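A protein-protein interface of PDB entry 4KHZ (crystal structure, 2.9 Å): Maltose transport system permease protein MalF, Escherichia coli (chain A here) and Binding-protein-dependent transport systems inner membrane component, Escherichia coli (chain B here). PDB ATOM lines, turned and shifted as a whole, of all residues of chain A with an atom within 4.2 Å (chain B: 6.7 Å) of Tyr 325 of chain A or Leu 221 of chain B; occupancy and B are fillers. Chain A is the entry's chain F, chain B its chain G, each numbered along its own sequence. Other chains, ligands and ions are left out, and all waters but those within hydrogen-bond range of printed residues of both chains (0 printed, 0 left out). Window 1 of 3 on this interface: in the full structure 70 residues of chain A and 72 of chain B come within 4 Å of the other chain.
Ile 322 of chain A touches Phe 278 of chain B (CG2 to CE2, 3.4 Å). Tyr 325 of chain A touches Leu 221 of chain B. Ile 224 of chain B touches Tyr 325 of chain A (CD1 to CE2, 3.6 Å). Tyr 325 of chain A touches Ile 274 of chain B (O to CG2, 3.9 Å). O of Ala 326 of chain A touches CD1 of Ile 274 of chain B, at 3.2 Å. Phe 278 of chain B touches Ala 326 of chain A. Tyr 383 of chain A touches Leu 221 of chain B.
Of chain B, only Leu 221 (3.9 Å), Ile 224 (3.6 Å) and Ile 274 (3.9 Å) come within 4 Å of Tyr 325 of chain A. Of chain A, only Tyr 325 and Tyr 383 come within 4 Å of Leu 221 of chain B. Of the printed residues of chain A, Ile 274 of chain B touches Tyr 325 and Ala 326. Of the printed residues of chain A, Phe 278 of chain B touches Ile 322 (3.4 Å) and Ala 326 (3.8 Å). The nearest printed residue of chain A that does not touch Ile 274 of chain B is Val 327 of chain A (5.0 Å).
Of the 15 printed residues of chain B, 4 touch a printed residue of chain A. Printed residues of chain B that touch a printed residue of chain A: Leu 221, Ile 224, Ile 274 and Phe 278. Of the 9 printed residues of chain A, 4 touch a printed residue of chain B. Hydrophobic or aromatic side chains of chain A within 4 Å of the printed part of chain B: Ile 322, Tyr 325, Ala 326 and Tyr 383. Among the printed residues, no Asp or Glu carboxylate lies within 4 Å of a Lys or Arg side-chain nitrogen of the other chain.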
ATOM      1  N   ILE A 322      16.419 -16.800 -24.747  1.00  0.00           N
ATOM      2  CA  ILE A 322      17.068 -17.103 -23.466  1.00  0.00           C
ATOM      3  C   ILE A 322      18.584 -17.278 -23.610  1.00  0.00           C
ATOM      4  O   ILE A 322      19.327 -17.023 -22.658  1.00  0.00           O
ATOM      5  CB  ILE A 322      16.440 -18.360 -22.818  1.00  0.00           C
ATOM      6  CG1 ILE A 322      15.038 -18.027 -22.299  1.00  0.00           C
ATOM      7  CG2 ILE A 322      17.291 -18.888 -21.666  1.00  0.00           C
ATOM      8  CD1 ILE A 322      14.232 -19.238 -21.877  1.00  0.00           C
ATOM      9  N   LEU A 323      19.039 -17.695 -24.793  1.00  0.00           N
ATOM     10  CA  LEU A 323      20.469 -17.952 -25.046  1.00  0.00           C
ATOM     11  C   LEU A 323      21.434 -16.888 -24.497  1.00  0.00           C
ATOM     12  O   LEU A 323      22.476 -17.241 -23.950  1.00  0.00           O
ATOM     13  CB  LEU A 323      20.732 -18.169 -26.543  1.00  0.00           C
ATOM     14  CG  LEU A 323      20.413 -19.564 -27.089  1.00  0.00           C
ATOM     15  CD1 LEU A 323      20.572 -19.589 -28.601  1.00  0.00           C
ATOM     16  CD2 LEU A 323      21.287 -20.631 -26.443  1.00  0.00           C
ATOM     17  N   PRO A 324      21.106 -15.592 -24.654  1.00  0.00           N
ATOM     18  CA  PRO A 324      21.942 -14.562 -24.033  1.00  0.00           C
ATOM     19  C   PRO A 324      22.219 -14.810 -22.551  1.00  0.00           C
ATOM     20  O   PRO A 324      23.350 -14.629 -22.101  1.00  0.00           O
ATOM     21  CB  PRO A 324      21.109 -13.293 -24.208  1.00  0.00           C
ATOM     22  CG  PRO A 324      20.362 -13.524 -25.472  1.00  0.00           C
ATOM     23  CD  PRO A 324      20.097 -15.002 -25.553  1.00  0.00           C
ATOM     24  N   TYR A 325      21.193 -15.237 -21.817  1.00  0.00           N
ATOM     25  CA  TYR A 325      21.312 -15.516 -20.380  1.00  0.00           C
ATOM     26  C   TYR A 325      22.188 -16.746 -20.114  1.00  0.00           C
ATOM     27  O   TYR A 325      22.772 -16.873 -19.038  1.00  0.00           O
ATOM     28  CB  TYR A 325      19.917 -15.701 -19.754  1.00  0.00           C
ATOM     29  CG  TYR A 325      19.774 -15.202 -18.323  1.00  0.00           C
ATOM     30  CD1 TYR A 325      20.211 -13.928 -17.955  1.00  0.00           C
ATOM     31  CD2 TYR A 325      19.167 -15.990 -17.347  1.00  0.00           C
ATOM     32  CE1 TYR A 325      20.071 -13.469 -16.654  1.00  0.00           C
ATOM     33  CE2 TYR A 325      19.022 -15.537 -16.043  1.00  0.00           C
ATOM     34  CZ  TYR A 325      19.478 -14.277 -15.702  1.00  0.00           C
ATOM     35  OH  TYR A 325      19.337 -13.821 -14.410  1.00  0.00           O
ATOM     36  N   ALA A 326      22.276 -17.643 -21.097  1.00  0.00           N
ATOM     37  CA  ALA A 326      23.161 -18.808 -21.017  1.00  0.00           C
ATOM     38  C   ALA A 326      24.638 -18.421 -21.134  1.00  0.00           C
ATOM     39  O   ALA A 326      25.514 -19.211 -20.786  1.00  0.00           O
ATOM     40  CB  ALA A 326      22.799 -19.830 -22.090  1.00  0.00           C
ATOM     41  N   VAL A 327      24.903 -17.215 -21.631  1.00  0.00           N
ATOM     42  CA  VAL A 327      26.259 -16.684 -21.734  1.00  0.00           C
ATOM     43  C   VAL A 327      26.561 -15.812 -20.509  1.00  0.00           C
ATOM     44  O   VAL A 327      25.831 -14.853 -20.241  1.00  0.00           O
ATOM     45  CB  VAL A 327      26.424 -15.846 -23.019  1.00  0.00           C
ATOM     46  CG1 VAL A 327      27.877 -15.437 -23.213  1.00  0.00           C
ATOM     47  CG2 VAL A 327      25.925 -16.627 -24.228  1.00  0.00           C
ATOM     48  N   LEU A 379      21.494  -7.991 -21.564  1.00  0.00           N
ATOM     49  CA  LEU A 379      21.763  -8.932 -20.478  1.00  0.00           C
ATOM     50  C   LEU A 379      20.547  -9.136 -19.574  1.00  0.00           C
ATOM     51  O   LEU A 379      20.340 -10.229 -19.043  1.00  0.00           O
ATOM     52  CB  LEU A 379      22.936  -8.446 -19.616  1.00  0.00           C
ATOM     53  CG  LEU A 379      24.360  -8.494 -20.176  1.00  0.00           C
ATOM     54  CD1 LEU A 379      24.662  -7.289 -21.048  1.00  0.00           C
ATOM     55  CD2 LEU A 379      25.358  -8.572 -19.031  1.00  0.00           C
ATOM     56  N   PRO A 382      16.298 -11.259 -20.475  1.00  0.00           N
ATOM     57  CA  PRO A 382      15.929 -12.659 -20.249  1.00  0.00           C
ATOM     58  C   PRO A 382      15.460 -12.945 -18.823  1.00  0.00           C
ATOM     59  O   PRO A 382      14.497 -13.684 -18.634  1.00  0.00           O
ATOM     60  CB  PRO A 382      17.220 -13.427 -20.562  1.00  0.00           C
ATOM     61  CG  PRO A 382      18.308 -12.411 -20.516  1.00  0.00           C
ATOM     62  CD  PRO A 382      17.673 -11.148 -20.994  1.00  0.00           C
ATOM     63  N   TYR A 383      16.130 -12.363 -17.833  1.00  0.00           N
ATOM     64  CA  TYR A 383      15.709 -12.515 -16.443  1.00  0.00           C
ATOM     65  C   TYR A 383      14.259 -12.077 -16.266  1.00  0.00           C
ATOM     66  O   TYR A 383      13.480 -12.758 -15.601  1.00  0.00           O
ATOM     67  CB  TYR A 383      16.618 -11.719 -15.503  1.00  0.00           C
ATOM     68  CG  TYR A 383      16.100 -11.638 -14.084  1.00  0.00           C
ATOM     69  CD1 TYR A 383      15.904 -12.788 -13.326  1.00  0.00           C
ATOM     70  CD2 TYR A 383      15.804 -10.412 -13.501  1.00  0.00           C
ATOM     71  CE1 TYR A 383      15.426 -12.719 -12.026  1.00  0.00           C
ATOM     72  CE2 TYR A 383      15.328 -10.331 -12.203  1.00  0.00           C
ATOM     73  CZ  TYR A 383      15.140 -11.485 -11.470  1.00  0.00           C
ATOM     74  OH  TYR A 383      14.667 -11.395 -10.182  1.00  0.00           O
ATOM     75  N   ALA B  96      25.002 -23.060  -5.400  1.00  0.00           N
ATOM     76  CA  ALA B  96      23.579 -22.989  -5.721  1.00  0.00           C
ATOM     77  C   ALA B  96      22.763 -23.983  -4.899  1.00  0.00           C
ATOM     78  O   ALA B  96      21.661 -23.658  -4.461  1.00  0.00           O
ATOM     79  CB  ALA B  96      23.360 -23.219  -7.208  1.00  0.00           C
ATOM     80  N   HIS B 173      16.161 -14.823  -2.099  1.00  0.00           N
ATOM     81  CA  HIS B 173      15.756 -16.220  -2.182  1.00  0.00           C
ATOM     82  C   HIS B 173      14.741 -16.557  -1.098  1.00  0.00           C
ATOM     83  O   HIS B 173      13.736 -17.218  -1.364  1.00  0.00           O
ATOM     84  CB  HIS B 173      16.977 -17.132  -2.075  1.00  0.00           C
ATOM     85  CG  HIS B 173      17.954 -16.956  -3.196  1.00  0.00           C
ATOM     86  ND1 HIS B 173      17.628 -17.206  -4.510  1.00  0.00           N
ATOM     87  CD2 HIS B 173      19.245 -16.548  -3.199  1.00  0.00           C
ATOM     88  CE1 HIS B 173      18.676 -16.965  -5.275  1.00  0.00           C
ATOM     89  NE2 HIS B 173      19.671 -16.565  -4.505  1.00  0.00           N
ATOM     90  N   ALA B 216      13.944 -25.227  -8.462  1.00  0.00           N
ATOM     91  CA  ALA B 216      14.687 -25.361  -9.713  1.00  0.00           C
ATOM     92  C   ALA B 216      15.066 -23.988 -10.269  1.00  0.00           C
ATOM     93  O   ALA B 216      16.192 -23.789 -10.728  1.00  0.00           O
ATOM     94  CB  ALA B 216      13.878 -26.147 -10.735  1.00  0.00           C
ATOM     95  N   VAL B 217      14.124 -23.046 -10.216  1.00  0.00           N
ATOM     96  CA  VAL B 217      14.380 -21.664 -10.631  1.00  0.00           C
ATOM     97  C   VAL B 217      15.467 -21.035  -9.756  1.00  0.00           C
ATOM     98  O   VAL B 217      16.475 -20.547 -10.269  1.00  0.00           O
ATOM     99  CB  VAL B 217      13.095 -20.804 -10.573  1.00  0.00           C
ATOM    100  CG1 VAL B 217      13.415 -19.319 -10.686  1.00  0.00           C
ATOM    101  CG2 VAL B 217      12.132 -21.218 -11.676  1.00  0.00           C
ATOM    102  N   VAL B 218      15.258 -21.061  -8.441  1.00  0.00           N
ATOM    103  CA  VAL B 218      16.216 -20.492  -7.486  1.00  0.00           C
ATOM    104  C   VAL B 218      17.622 -21.039  -7.727  1.00  0.00           C
ATOM    105  O   VAL B 218      18.590 -20.277  -7.743  1.00  0.00           O
ATOM    106  CB  VAL B 218      15.795 -20.762  -6.019  1.00  0.00           C
ATOM    107  CG1 VAL B 218      16.936 -20.460  -5.049  1.00  0.00           C
ATOM    108  CG2 VAL B 218      14.561 -19.944  -5.654  1.00  0.00           C
ATOM    109  N   PHE B 219      17.727 -22.355  -7.911  1.00  0.00           N
ATOM    110  CA  PHE B 219      19.014 -22.998  -8.189  1.00  0.00           C
ATOM    111  C   PHE B 219      19.691 -22.378  -9.412  1.00  0.00           C
ATOM    112  O   PHE B 219      20.868 -22.026  -9.365  1.00  0.00           O
ATOM    113  CB  PHE B 219      18.839 -24.508  -8.399  1.00  0.00           C
ATOM    114  CG  PHE B 219      20.077 -25.195  -8.906  1.00  0.00           C
ATOM    115  CD1 PHE B 219      21.066 -25.614  -8.026  1.00  0.00           C
ATOM    116  CD2 PHE B 219      20.260 -25.414 -10.264  1.00  0.00           C
ATOM    117  CE1 PHE B 219      22.210 -26.240  -8.495  1.00  0.00           C
ATOM    118  CE2 PHE B 219      21.402 -26.039 -10.738  1.00  0.00           C
ATOM    119  CZ  PHE B 219      22.379 -26.452  -9.852  1.00  0.00           C
ATOM    120  N   ILE B 220      18.936 -22.242 -10.497  1.00  0.00           N
ATOM    121  CA  ILE B 220      19.475 -21.711 -11.748  1.00  0.00           C
ATOM    122  C   ILE B 220      19.949 -20.266 -11.583  1.00  0.00           C
ATOM    123  O   ILE B 220      21.034 -19.916 -12.040  1.00  0.00           O
ATOM    124  CB  ILE B 220      18.440 -21.808 -12.888  1.00  0.00           C
ATOM    125  CG1 ILE B 220      18.190 -23.280 -13.236  1.00  0.00           C
ATOM    126  CG2 ILE B 220      18.917 -21.056 -14.123  1.00  0.00           C
ATOM    127  CD1 ILE B 220      16.892 -23.536 -13.971  1.00  0.00           C
ATOM    128  N   LEU B 221      19.139 -19.441 -10.924  1.00  0.00           N
ATOM    129  CA  LEU B 221      19.486 -18.041 -10.682  1.00  0.00           C
ATOM    130  C   LEU B 221      20.727 -17.916  -9.798  1.00  0.00           C
ATOM    131  O   LEU B 221      21.578 -17.053 -10.031  1.00  0.00           O
ATOM    132  CB  LEU B 221      18.308 -17.297 -10.047  1.00  0.00           C
ATOM    133  CG  LEU B 221      17.056 -17.173 -10.919  1.00  0.00           C
ATOM    134  CD1 LEU B 221      15.870 -16.695 -10.096  1.00  0.00           C
ATOM    135  CD2 LEU B 221      17.301 -16.244 -12.098  1.00  0.00           C
ATOM    136  N   SER B 222      20.824 -18.777  -8.788  1.00  0.00           N
ATOM    137  CA  SER B 222      22.020 -18.853  -7.949  1.00  0.00           C
ATOM    138  C   SER B 222      23.209 -19.386  -8.744  1.00  0.00           C
ATOM    139  O   SER B 222      24.334 -18.922  -8.570  1.00  0.00           O
ATOM    140  CB  SER B 222      21.777 -19.752  -6.735  1.00  0.00           C
ATOM    141  OG  SER B 222      20.667 -19.304  -5.979  1.00  0.00           O
ATOM    142  N   PHE B 223      22.954 -20.364  -9.613  1.00  0.00           N
ATOM    143  CA  PHE B 223      24.001 -20.962 -10.434  1.00  0.00           C
ATOM    144  C   PHE B 223      24.562 -19.944 -11.419  1.00  0.00           C
ATOM    145  O   PHE B 223      25.775 -19.776 -11.527  1.00  0.00           O
ATOM    146  CB  PHE B 223      23.462 -22.177 -11.191  1.00  0.00           C
ATOM    147  CG  PHE B 223      24.500 -22.895 -12.002  1.00  0.00           C
ATOM    148  CD1 PHE B 223      25.397 -23.760 -11.393  1.00  0.00           C
ATOM    149  CD2 PHE B 223      24.582 -22.708 -13.373  1.00  0.00           C
ATOM    150  CE1 PHE B 223      26.356 -24.426 -12.135  1.00  0.00           C
ATOM    151  CE2 PHE B 223      25.541 -23.370 -14.122  1.00  0.00           C
ATOM    152  CZ  PHE B 223      26.429 -24.232 -13.501  1.00  0.00           C
ATOM    153  N   ILE B 224      23.668 -19.265 -12.128  1.00  0.00           N
ATOM    154  CA  ILE B 224      24.060 -18.236 -13.090  1.00  0.00           C
ATOM    155  C   ILE B 224      24.805 -17.104 -12.385  1.00  0.00           C
ATOM    156  O   ILE B 224      25.816 -16.607 -12.887  1.00  0.00           O
ATOM    157  CB  ILE B 224      22.833 -17.684 -13.846  1.00  0.00           C
ATOM    158  CG1 ILE B 224      22.269 -18.760 -14.780  1.00  0.00           C
ATOM    159  CG2 ILE B 224      23.203 -16.443 -14.653  1.00  0.00           C
ATOM    160  CD1 ILE B 224      20.845 -18.509 -15.224  1.00  0.00           C
ATOM    161  N   ALA B 225      24.304 -16.711 -11.217  1.00  0.00           N
ATOM    162  CA  ALA B 225      24.950 -15.680 -10.413  1.00  0.00           C
ATOM    163  C   ALA B 225      26.399 -16.051 -10.108  1.00  0.00           C
ATOM    164  O   ALA B 225      27.301 -15.234 -10.284  1.00  0.00           O
ATOM    165  CB  ALA B 225      24.176 -15.452  -9.123  1.00  0.00           C
ATOM    166  N   ALA B 226      26.617 -17.290  -9.675  1.00  0.00           N
ATOM    167  CA  ALA B 226      27.948 -17.748  -9.276  1.00  0.00           C
ATOM    168  C   ALA B 226      28.905 -17.901 -10.460  1.00  0.00           C
ATOM    169  O   ALA B 226      30.099 -17.629 -10.335  1.00  0.00           O
ATOM    170  CB  ALA B 226      27.845 -19.056  -8.514  1.00  0.00           C
ATOM    171  N   ILE B 274      25.563 -23.286 -18.333  1.00  0.00           N
ATOM    172  CA  ILE B 274      24.223 -22.720 -18.131  1.00  0.00           C
ATOM    173  C   ILE B 274      23.230 -23.281 -19.156  1.00  0.00           C
ATOM    174  O   ILE B 274      22.041 -23.431 -18.859  1.00  0.00           O
ATOM    175  CB  ILE B 274      24.220 -21.172 -18.201  1.00  0.00           C
ATOM    176  CG1 ILE B 274      25.283 -20.578 -17.268  1.00  0.00           C
ATOM    177  CG2 ILE B 274      22.851 -20.615 -17.833  1.00  0.00           C
ATOM    178  CD1 ILE B 274      26.587 -20.220 -17.954  1.00  0.00           C
ATOM    179  N   PHE B 278      19.803 -25.248 -18.481  1.00  0.00           N
ATOM    180  CA  PHE B 278      18.508 -24.965 -19.114  1.00  0.00           C
ATOM    181  C   PHE B 278      17.929 -26.219 -19.761  1.00  0.00           C
ATOM    182  O   PHE B 278      16.733 -26.491 -19.637  1.00  0.00           O
ATOM    183  CB  PHE B 278      18.624 -23.877 -20.191  1.00  0.00           C
ATOM    184  CG  PHE B 278      18.784 -22.478 -19.655  1.00  0.00           C
ATOM    185  CD1 PHE B 278      18.045 -22.028 -18.564  1.00  0.00           C
ATOM    186  CD2 PHE B 278      19.645 -21.586 -20.283  1.00  0.00           C
ATOM    187  CE1 PHE B 278      18.191 -20.733 -18.092  1.00  0.00           C
ATOM    188  CE2 PHE B 278      19.791 -20.290 -19.816  1.00  0.00           C
ATOM    189  CZ  PHE B 278      19.064 -19.864 -18.719  1.00  0.00           C
